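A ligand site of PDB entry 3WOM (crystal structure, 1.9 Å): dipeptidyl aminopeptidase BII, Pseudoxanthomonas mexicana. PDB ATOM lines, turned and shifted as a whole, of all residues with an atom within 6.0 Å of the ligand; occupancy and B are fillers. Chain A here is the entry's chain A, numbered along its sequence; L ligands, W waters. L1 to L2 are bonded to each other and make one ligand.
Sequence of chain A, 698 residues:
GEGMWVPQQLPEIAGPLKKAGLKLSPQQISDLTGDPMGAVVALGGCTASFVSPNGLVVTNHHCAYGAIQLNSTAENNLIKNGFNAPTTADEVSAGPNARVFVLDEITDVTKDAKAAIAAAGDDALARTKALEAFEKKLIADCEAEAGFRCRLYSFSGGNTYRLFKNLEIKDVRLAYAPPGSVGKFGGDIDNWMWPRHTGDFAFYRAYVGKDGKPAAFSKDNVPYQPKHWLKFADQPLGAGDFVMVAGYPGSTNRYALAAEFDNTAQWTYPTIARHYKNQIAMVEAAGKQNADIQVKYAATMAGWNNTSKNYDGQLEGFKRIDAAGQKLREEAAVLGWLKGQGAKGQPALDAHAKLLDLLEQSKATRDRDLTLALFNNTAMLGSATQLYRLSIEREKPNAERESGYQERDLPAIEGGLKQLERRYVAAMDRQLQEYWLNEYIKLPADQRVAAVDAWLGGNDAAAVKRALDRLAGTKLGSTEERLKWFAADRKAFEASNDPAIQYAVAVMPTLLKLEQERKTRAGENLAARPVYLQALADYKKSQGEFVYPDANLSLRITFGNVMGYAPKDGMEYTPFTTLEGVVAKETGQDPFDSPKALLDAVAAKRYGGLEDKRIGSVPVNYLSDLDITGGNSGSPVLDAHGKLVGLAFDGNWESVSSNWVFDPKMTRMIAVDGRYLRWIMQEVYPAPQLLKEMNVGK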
ATOM      1  N   GLY A  45     -18.679   2.947  17.103  1.00  0.00           N
ATOM      2  CA  GLY A  45     -18.435   1.725  17.826  1.00  0.00           C
ATOM      3  C   GLY A  45     -18.389   1.766  19.378  1.00  0.00           C
ATOM      4  O   GLY A  45     -18.312   0.703  20.043  1.00  0.00           O
ATOM      5  N   CYS A  46     -18.374   2.957  19.944  1.00  0.00           N
ATOM      6  CA  CYS A  46     -18.605   3.168  21.406  1.00  0.00           C
ATOM      7  C   CYS A  46     -19.516   4.390  21.532  1.00  0.00           C
ATOM      8  O   CYS A  46     -19.683   5.125  20.593  1.00  0.00           O
ATOM      9  CB  CYS A  46     -17.272   3.462  22.091  1.00  0.00           C
ATOM     10  SG  CYS A  46     -16.378   1.919  22.763  1.00  0.00           S
ATOM     11  N   ASN A  60     -15.461   4.899  28.210  1.00  0.00           N
ATOM     12  CA  ASN A  60     -14.720   3.900  28.860  1.00  0.00           C
ATOM     13  C   ASN A  60     -13.261   3.931  28.461  1.00  0.00           C
ATOM     14  O   ASN A  60     -12.918   4.338  27.330  1.00  0.00           O
ATOM     15  CB  ASN A  60     -15.231   2.513  28.516  1.00  0.00           C
ATOM     16  CG  ASN A  60     -16.614   2.209  29.034  1.00  0.00           C
ATOM     17  OD1 ASN A  60     -17.178   2.794  30.023  1.00  0.00           O
ATOM     18  ND2 ASN A  60     -17.140   1.215  28.447  1.00  0.00           N
ATOM     19  N   HIS A  62     -11.618   1.118  27.855  1.00  0.00           N
ATOM     20  CA  HIS A  62     -11.473   0.200  26.730  1.00  0.00           C
ATOM     21  C   HIS A  62     -11.871   0.869  25.420  1.00  0.00           C
ATOM     22  O   HIS A  62     -11.436   0.431  24.353  1.00  0.00           O
ATOM     23  CB  HIS A  62     -12.111  -1.174  26.975  1.00  0.00           C
ATOM     24  CG  HIS A  62     -13.601  -1.213  26.812  1.00  0.00           C
ATOM     25  ND1 HIS A  62     -14.457  -1.059  27.873  1.00  0.00           N
ATOM     26  CD2 HIS A  62     -14.378  -1.378  25.723  1.00  0.00           C
ATOM     27  CE1 HIS A  62     -15.699  -1.188  27.460  1.00  0.00           C
ATOM     28  NE2 HIS A  62     -15.681  -1.361  26.158  1.00  0.00           N
ATOM     29  N   CYS A  63     -12.747   1.904  25.467  1.00  0.00           N
ATOM     30  CA  CYS A  63     -13.040   2.669  24.291  1.00  0.00           C
ATOM     31  C   CYS A  63     -11.905   3.589  23.863  1.00  0.00           C
ATOM     32  O   CYS A  63     -11.741   3.854  22.632  1.00  0.00           O
ATOM     33  CB  CYS A  63     -14.355   3.516  24.495  1.00  0.00           C
ATOM     34  SG  CYS A  63     -15.801   2.461  24.792  1.00  0.00           S
ATOM     35  N   ASN A 191     -13.103 -10.052  32.400  1.00  0.00           N
ATOM     36  CA  ASN A 191     -13.917  -9.731  31.246  1.00  0.00           C
ATOM     37  C   ASN A 191     -15.103 -10.644  31.125  1.00  0.00           C
ATOM     38  O   ASN A 191     -14.987 -11.865  31.325  1.00  0.00           O
ATOM     39  CB  ASN A 191     -13.046  -9.769  29.972  1.00  0.00           C
ATOM     40  CG  ASN A 191     -13.677  -9.015  28.825  1.00  0.00           C
ATOM     41  OD1 ASN A 191     -14.507  -8.080  29.031  1.00  0.00           O
ATOM     42  ND2 ASN A 191     -13.402  -9.505  27.622  1.00  0.00           N
ATOM     43  N   TRP A 192     -16.264 -10.036  30.832  1.00  0.00           N
ATOM     44  CA  TRP A 192     -17.579 -10.706  30.809  1.00  0.00           C
ATOM     45  C   TRP A 192     -17.967 -11.277  32.097  1.00  0.00           C
ATOM     46  O   TRP A 192     -18.808 -12.172  32.102  1.00  0.00           O
ATOM     47  CB  TRP A 192     -17.676 -11.761  29.755  1.00  0.00           C
ATOM     48  CG  TRP A 192     -17.376 -11.212  28.397  1.00  0.00           C
ATOM     49  CD1 TRP A 192     -16.277 -11.452  27.643  1.00  0.00           C
ATOM     50  CD2 TRP A 192     -18.211 -10.317  27.606  1.00  0.00           C
ATOM     51  NE1 TRP A 192     -16.390 -10.784  26.399  1.00  0.00           N
ATOM     52  CE2 TRP A 192     -17.553 -10.087  26.387  1.00  0.00           C
ATOM     53  CE3 TRP A 192     -19.434  -9.771  27.794  1.00  0.00           C
ATOM     54  CZ2 TRP A 192     -18.077  -9.260  25.393  1.00  0.00           C
ATOM     55  CZ3 TRP A 192     -19.943  -8.946  26.827  1.00  0.00           C
ATOM     56  CH2 TRP A 192     -19.262  -8.659  25.656  1.00  0.00           C
ATOM     57  N   ARG A 196     -17.267  -7.656  39.533  1.00  0.00           N
ATOM     58  CA  ARG A 196     -16.422  -6.893  38.667  1.00  0.00           C
ATOM     59  C   ARG A 196     -15.875  -5.699  39.497  1.00  0.00           C
ATOM     60  O   ARG A 196     -16.613  -5.097  40.352  1.00  0.00           O
ATOM     61  CB  ARG A 196     -17.143  -6.432  37.418  1.00  0.00           C
ATOM     62  CG  ARG A 196     -16.221  -5.931  36.342  1.00  0.00           C
ATOM     63  CD  ARG A 196     -15.237  -6.968  35.877  1.00  0.00           C
ATOM     64  NE  ARG A 196     -14.770  -6.603  34.542  1.00  0.00           N
ATOM     65  CZ  ARG A 196     -15.448  -6.769  33.424  1.00  0.00           C
ATOM     66  NH1 ARG A 196     -16.665  -7.365  33.469  1.00  0.00           N
ATOM     67  NH2 ARG A 196     -14.928  -6.369  32.233  1.00  0.00           N
ATOM     68  N   ASP A 200     -13.372   1.351  34.509  1.00  0.00           N
ATOM     69  CA  ASP A 200     -13.354   1.466  33.061  1.00  0.00           C
ATOM     70  C   ASP A 200     -13.859   2.845  32.544  1.00  0.00           C
ATOM     71  O   ASP A 200     -15.006   3.005  32.128  1.00  0.00           O
ATOM     72  CB  ASP A 200     -14.160   0.288  32.492  1.00  0.00           C
ATOM     73  CG  ASP A 200     -13.803   0.014  31.026  1.00  0.00           C
ATOM     74  OD1 ASP A 200     -13.108   0.878  30.427  1.00  0.00           O
ATOM     75  OD2 ASP A 200     -14.195  -1.029  30.546  1.00  0.00           O
ATOM     76  N   ASN A 306     -11.601 -10.277  23.694  1.00  0.00           N
ATOM     77  CA  ASN A 306     -12.980  -9.907  24.017  1.00  0.00           C
ATOM     78  C   ASN A 306     -14.015 -10.712  23.203  1.00  0.00           C
ATOM     79  O   ASN A 306     -14.960 -11.315  23.739  1.00  0.00           O
ATOM     80  CB  ASN A 306     -13.174  -8.429  23.731  1.00  0.00           C
ATOM     81  CG  ASN A 306     -14.473  -7.912  24.296  1.00  0.00           C
ATOM     82  OD1 ASN A 306     -14.814  -8.246  25.420  1.00  0.00           O
ATOM     83  ND2 ASN A 306     -15.228  -7.172  23.529  1.00  0.00           N
ATOM     84  N   ASN A 310     -16.457 -13.714  24.416  1.00  0.00           N
ATOM     85  CA  ASN A 310     -17.857 -13.488  24.206  1.00  0.00           C
ATOM     86  C   ASN A 310     -18.506 -14.665  23.566  1.00  0.00           C
ATOM     87  O   ASN A 310     -19.529 -15.128  23.985  1.00  0.00           O
ATOM     88  CB  ASN A 310     -18.091 -12.276  23.296  1.00  0.00           C
ATOM     89  CG  ASN A 310     -19.580 -12.031  23.078  1.00  0.00           C
ATOM     90  OD1 ASN A 310     -20.276 -11.272  23.811  1.00  0.00           O
ATOM     91  ND2 ASN A 310     -20.098 -12.660  22.188  1.00  0.00           N
ATOM     92  N   ILE A 628     -28.381  -3.822  27.028  1.00  0.00           N
ATOM     93  CA  ILE A 628     -27.327  -3.228  26.253  1.00  0.00           C
ATOM     94  C   ILE A 628     -26.488  -4.328  25.542  1.00  0.00           C
ATOM     95  O   ILE A 628     -26.526  -5.506  25.861  1.00  0.00           O
ATOM     96  CB  ILE A 628     -26.361  -2.320  27.067  1.00  0.00           C
ATOM     97  CG1 ILE A 628     -25.611  -3.085  28.196  1.00  0.00           C
ATOM     98  CG2 ILE A 628     -27.106  -1.179  27.665  1.00  0.00           C
ATOM     99  CD1 ILE A 628     -24.345  -2.381  28.677  1.00  0.00           C
ATOM    100  N   THR A 629     -25.700  -3.866  24.590  1.00  0.00           N
ATOM    101  CA  THR A 629     -24.761  -4.747  23.878  1.00  0.00           C
ATOM    102  C   THR A 629     -23.590  -3.989  23.271  1.00  0.00           C
ATOM    103  O   THR A 629     -23.475  -2.773  23.503  1.00  0.00           O
ATOM    104  CB  THR A 629     -25.574  -5.591  22.854  1.00  0.00           C
ATOM    105  OG1 THR A 629     -24.708  -6.651  22.438  1.00  0.00           O
ATOM    106  CG2 THR A 629     -25.913  -4.858  21.711  1.00  0.00           C
ATOM    107  N   GLY A 630     -22.722  -4.645  22.490  1.00  0.00           N
ATOM    108  CA  GLY A 630     -21.537  -4.052  21.839  1.00  0.00           C
ATOM    109  C   GLY A 630     -21.937  -2.717  21.174  1.00  0.00           C
ATOM    110  O   GLY A 630     -22.962  -2.654  20.505  1.00  0.00           O
ATOM    111  N   GLY A 631     -21.193  -1.668  21.470  1.00  0.00           N
ATOM    112  CA  GLY A 631     -21.458  -0.294  20.998  1.00  0.00           C
ATOM    113  C   GLY A 631     -21.982   0.588  22.149  1.00  0.00           C
ATOM    114  O   GLY A 631     -21.841   1.805  22.073  1.00  0.00           O
ATOM    115  N   ASN A 632     -22.580  -0.034  23.180  1.00  0.00           N
ATOM    116  CA  ASN A 632     -23.057   0.704  24.385  1.00  0.00           C
ATOM    117  C   ASN A 632     -21.952   1.015  25.349  1.00  0.00           C
ATOM    118  O   ASN A 632     -22.183   1.806  26.293  1.00  0.00           O
ATOM    119  CB  ASN A 632     -24.204  -0.027  25.164  1.00  0.00           C
ATOM    120  CG  ASN A 632     -25.593   0.370  24.713  1.00  0.00           C
ATOM    121  OD1 ASN A 632     -26.050   1.573  24.847  1.00  0.00           O
ATOM    122  ND2 ASN A 632     -26.344  -0.594  24.257  1.00  0.00           N
ATOM    123  N   SER A 633     -20.812   0.350  25.262  1.00  0.00           N
ATOM    124  CA  SER A 633     -19.705   0.744  26.085  1.00  0.00           C
ATOM    125  C   SER A 633     -19.524   2.255  26.057  1.00  0.00           C
ATOM    126  O   SER A 633     -19.570   2.836  24.975  1.00  0.00           O
ATOM    127  CB  SER A 633     -18.402   0.079  25.687  1.00  0.00           C
ATOM    128  OG  SER A 633     -18.417  -1.198  26.393  1.00  0.00           O
ATOM    129  N   PHE A 649     -20.285  -0.430  30.819  1.00  0.00           N
ATOM    130  CA  PHE A 649     -19.091  -1.063  30.176  1.00  0.00           C
ATOM    131  C   PHE A 649     -19.141  -2.518  29.765  1.00  0.00           C
ATOM    132  O   PHE A 649     -18.332  -2.912  28.891  1.00  0.00           O
ATOM    133  CB  PHE A 649     -17.749  -0.735  30.915  1.00  0.00           C
ATOM    134  CG  PHE A 649     -17.506  -1.496  32.219  1.00  0.00           C
ATOM    135  CD1 PHE A 649     -18.025  -1.002  33.437  1.00  0.00           C
ATOM    136  CD2 PHE A 649     -16.669  -2.602  32.267  1.00  0.00           C
ATOM    137  CE1 PHE A 649     -17.797  -1.588  34.650  1.00  0.00           C
ATOM    138  CE2 PHE A 649     -16.381  -3.165  33.518  1.00  0.00           C
ATOM    139  CZ  PHE A 649     -16.934  -2.653  34.722  1.00  0.00           C
ATOM    140  N   ASP A 650     -19.954  -3.381  30.381  1.00  0.00           N
ATOM    141  CA  ASP A 650     -19.888  -4.825  30.137  1.00  0.00           C
ATOM    142  C   ASP A 650     -21.213  -5.451  30.474  1.00  0.00           C
ATOM    143  O   ASP A 650     -22.150  -4.757  30.886  1.00  0.00           O
ATOM    144  CB  ASP A 650     -18.709  -5.468  30.926  1.00  0.00           C
ATOM    145  CG  ASP A 650     -18.134  -6.743  30.249  1.00  0.00           C
ATOM    146  OD1 ASP A 650     -18.728  -7.219  29.230  1.00  0.00           O
ATOM    147  OD2 ASP A 650     -17.181  -7.315  30.778  1.00  0.00           O
ATOM    148  N   GLY A 651     -21.325  -6.750  30.188  1.00  0.00           N
ATOM    149  CA  GLY A 651     -22.369  -7.617  30.686  1.00  0.00           C
ATOM    150  C   GLY A 651     -21.847  -8.820  31.401  1.00  0.00           C
ATOM    151  O   GLY A 651     -20.670  -9.202  31.239  1.00  0.00           O
ATOM    152  N   ASN A 652     -22.671  -9.343  32.321  1.00  0.00           N
ATOM    153  CA  ASN A 652     -22.325 -10.559  33.024  1.00  0.00           C
ATOM    154  C   ASN A 652     -22.293 -11.797  32.079  1.00  0.00           C
ATOM    155  O   ASN A 652     -22.774 -11.756  30.988  1.00  0.00           O
ATOM    156  CB  ASN A 652     -23.288 -10.794  34.200  1.00  0.00           C
ATOM    157  CG  ASN A 652     -24.713 -10.941  33.735  1.00  0.00           C
ATOM    158  OD1 ASN A 652     -25.334  -9.990  33.233  1.00  0.00           O
ATOM    159  ND2 ASN A 652     -25.202 -12.189  33.764  1.00  0.00           N
ATOM    160  N   SER A 655     -25.337 -13.258  30.396  1.00  0.00           N
ATOM    161  CA  SER A 655     -26.102 -12.344  29.616  1.00  0.00           C
ATOM    162  C   SER A 655     -25.868 -12.450  28.137  1.00  0.00           C
ATOM    163  O   SER A 655     -26.674 -11.924  27.381  1.00  0.00           O
ATOM    164  CB  SER A 655     -25.867 -10.891  30.008  1.00  0.00           C
ATOM    165  OG  SER A 655     -24.598 -10.378  29.556  1.00  0.00           O
ATOM    166  N   VAL A 656     -24.691 -12.930  27.753  1.00  0.00           N
ATOM    167  CA  VAL A 656     -24.239 -12.621  26.364  1.00  0.00           C
ATOM    168  C   VAL A 656     -25.096 -13.381  25.291  1.00  0.00           C
ATOM    169  O   VAL A 656     -25.263 -12.871  24.164  1.00  0.00           O
ATOM    170  CB  VAL A 656     -22.749 -12.912  26.160  1.00  0.00           C
ATOM    171  CG1 VAL A 656     -21.937 -11.866  26.930  1.00  0.00           C
ATOM    172  CG2 VAL A 656     -22.358 -14.350  26.629  1.00  0.00           C
ATOM    173  N   ARG A 668     -27.878  -8.695  32.736  1.00  0.00           N
ATOM    174  CA  ARG A 668     -27.592  -7.471  33.468  1.00  0.00           C
ATOM    175  C   ARG A 668     -26.506  -6.655  32.740  1.00  0.00           C
ATOM    176  O   ARG A 668     -25.596  -7.222  32.149  1.00  0.00           O
ATOM    177  CB  ARG A 668     -27.107  -7.831  34.837  1.00  0.00           C
ATOM    178  CG  ARG A 668     -28.105  -8.558  35.731  1.00  0.00           C
ATOM    179  CD  ARG A 668     -29.253  -7.651  36.089  1.00  0.00           C
ATOM    180  NE  ARG A 668     -30.197  -8.348  36.968  1.00  0.00           N
ATOM    181  CZ  ARG A 668     -31.214  -9.122  36.565  1.00  0.00           C
ATOM    182  NH1 ARG A 668     -31.526  -9.288  35.312  1.00  0.00           N
ATOM    183  NH2 ARG A 668     -31.971  -9.739  37.488  1.00  0.00           N
ATOM    184  N   MET A 669     -26.638  -5.356  32.814  1.00  0.00           N
ATOM    185  CA  MET A 669     -25.552  -4.405  32.595  1.00  0.00           C
ATOM    186  C   MET A 669     -24.605  -4.320  33.759  1.00  0.00           C
ATOM    187  O   MET A 669     -25.036  -4.328  34.935  1.00  0.00           O
ATOM    188  CB  MET A 669     -26.117  -3.015  32.281  1.00  0.00           C
ATOM    189  CG  MET A 669     -25.087  -1.886  32.389  1.00  0.00           C
ATOM    190  SD  MET A 669     -25.596  -0.257  31.771  1.00  0.00           S
ATOM    191  CE  MET A 669     -26.532   0.256  33.277  1.00  0.00           C
HETATM  192  N1  LIG L   1     -16.547  -7.002  27.495  1.00  0.00           N
HETATM  193  C1  LIG L   1     -16.753  -5.533  27.384  1.00  0.00           C
HETATM  194  C2  LIG L   1     -17.484  -5.226  26.071  1.00  0.00           C
HETATM  195  O1  LIG L   1     -17.355  -5.929  25.052  1.00  0.00           O
HETATM  196  C3  LIG L   1     -15.471  -4.688  27.574  1.00  0.00           C
HETATM  197  C4  LIG L   1     -14.951  -4.807  29.001  1.00  0.00           C
HETATM  198  C5  LIG L   1     -14.362  -5.073  26.576  1.00  0.00           C
HETATM  199  N1  LG2 L   2     -18.344  -4.245  26.149  1.00  0.00           N
HETATM  200  C1  LG2 L   2     -19.145  -3.884  25.014  1.00  0.00           C
HETATM  201  C2  LG2 L   2     -18.515  -2.843  24.136  1.00  0.00           C
HETATM  202  O1  LG2 L   2     -19.232  -2.046  23.559  1.00  0.00           O
HETATM  203  C3  LG2 L   2     -20.521  -3.375  25.562  1.00  0.00           C
HETATM  204  C4  LG2 L   2     -21.413  -4.580  25.941  1.00  0.00           C
HETATM  205  C5  LG2 L   2     -21.521  -5.686  25.137  1.00  0.00           C
HETATM  206  C6  LG2 L   2     -22.149  -4.597  27.164  1.00  0.00           C
HETATM  207  C7  LG2 L   2     -22.384  -6.748  25.479  1.00  0.00           C
HETATM  208  C8  LG2 L   2     -22.952  -5.672  27.507  1.00  0.00           C
HETATM  209  C9  LG2 L   2     -23.074  -6.740  26.713  1.00  0.00           C
HETATM  210  O2  LG2 L   2     -23.942  -7.795  27.070  1.00  0.00           O
HETATM  211  O3  LG2 L   2     -17.308  -2.626  24.156  1.00  0.00           O
HETATM  212  O   HOH W   1     -18.701  -6.856  22.579  1.00  0.00           O
HETATM  213  O   HOH W   2     -10.918  -5.356  26.560  1.00  0.00           O
HETATM  214  O   HOH W   3     -16.857  -1.347  21.919  1.00  0.00           O
HETATM  215  O   HOH W   4     -25.585  -6.973  29.436  1.00  0.00           O
HETATM  216  O   HOH W   5     -25.009  -9.035  24.425  1.00  0.00           O
HETATM  217  O   HOH W   6     -21.420  -7.242  22.025  1.00  0.00           O
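OD1 of Asn 191 sits at hydrogen-bond distance from N1 of LIG L1 (2.8 Å). An oxygen (O1) of LG2 L2 lies close to the backbone NH (N) of Ser 633, 3.3 Å away. O3 of LG2 L2 sits close to OG of Ser 633. The side-chain carboxylate (OD1) of Asp 650 is in salt-bridge range of a nitrogen (N1) of LIG L1, 2.8 Å away. An oxygen (O3) of LG2 L2 is in hydrogen-bond range of a ring nitrogen (NE2) of His 62 (2.9 Å). The backbone NH of Gly 631 sits at hydrogen-bond distance from an oxygen (O1) of LG2 L2, at 2.9 Å. The side-chain amide nitrogen of Asn 306 is in hydrogen-bond range of an oxygen (O1) of LIG L1 (2.9 Å). The backbone carbonyl oxygen (O) of Phe 649 sits at hydrogen-bond distance from a nitrogen (N1) of LG2 L2 (3.0 Å).
A ring nitrogen (NE2) of His 62 sits at hydrogen-bond distance from the side-chain hydroxyl (OG) of Ser 633, at 2.8 Å. OG of Ser 633 lies within hydrogen-bond range of O of Phe 649 (3.0 Å). The side-chain hydroxyl (OG) of Ser 633 lies close to the side-chain amide nitrogen (ND2) of Asn 60, 3.4 Å away. The side-chain carboxylate (OD2) of Asp 650 is in hydrogen-bond range of the backbone NH (N) of Trp 192 (2.9 Å). OD2 of Asp 200 lies within hydrogen-bond range of ND1 of His 62, at 2.7 Å. N of Thr 629 lies close to ND2 of Asn 632 (3.4 Å). OG of Ser 655 is in hydrogen-bond range of O of Asn 652, at 2.7 Å. SG of Cys 46 is disulfide-bonded to SG of Cys 63, at 2.2 Å.
Residues that only touch the ligand: Trp 192 (3.4 Å), Arg 196 (3.6 Å), Ile 628 (3.5 Å), Thr 629 (3.3 Å), Gly 630 (3.1 Å), Asn 632 (3.9 Å), Gly 651 (3.3 Å) and Ser 655 (3.6 Å). Hydrophobic or aromatic side chains within 4 Å of the ligand: His 62, Trp 192 and Ile 628. Within 4 Å of the ligand: His 62, Asn 191, Trp 192, Arg 196, Asn 306, Ile 628, Thr 629, Gly 630, Gly 631, Asn 632, Ser 633, Phe 649, Asp 650, Gly 651 and Ser 655.
Water W3 lies within hydrogen-bond range of an oxygen (O3) of LG2 L2 (2.6 Å), the backbone carbonyl oxygen of Gly 45 (3.1 Å) and the side-chain sulfur of Cys 46 (3.4 Å). Water W4 bridges O of Arg 668 (2.7 Å) and O2 of LG2 L2 (3.0 Å). Water W5 lies within hydrogen-bond range of O2 of LG2 L2 (3.1 Å) and OG1 of Thr 629 (3.1 Å). Water W6 bridges the backbone NH (N) of Gly 630 (2.9 Å) and the side-chain hydroxyl (OG1) of Thr 629 (3.4 Å).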
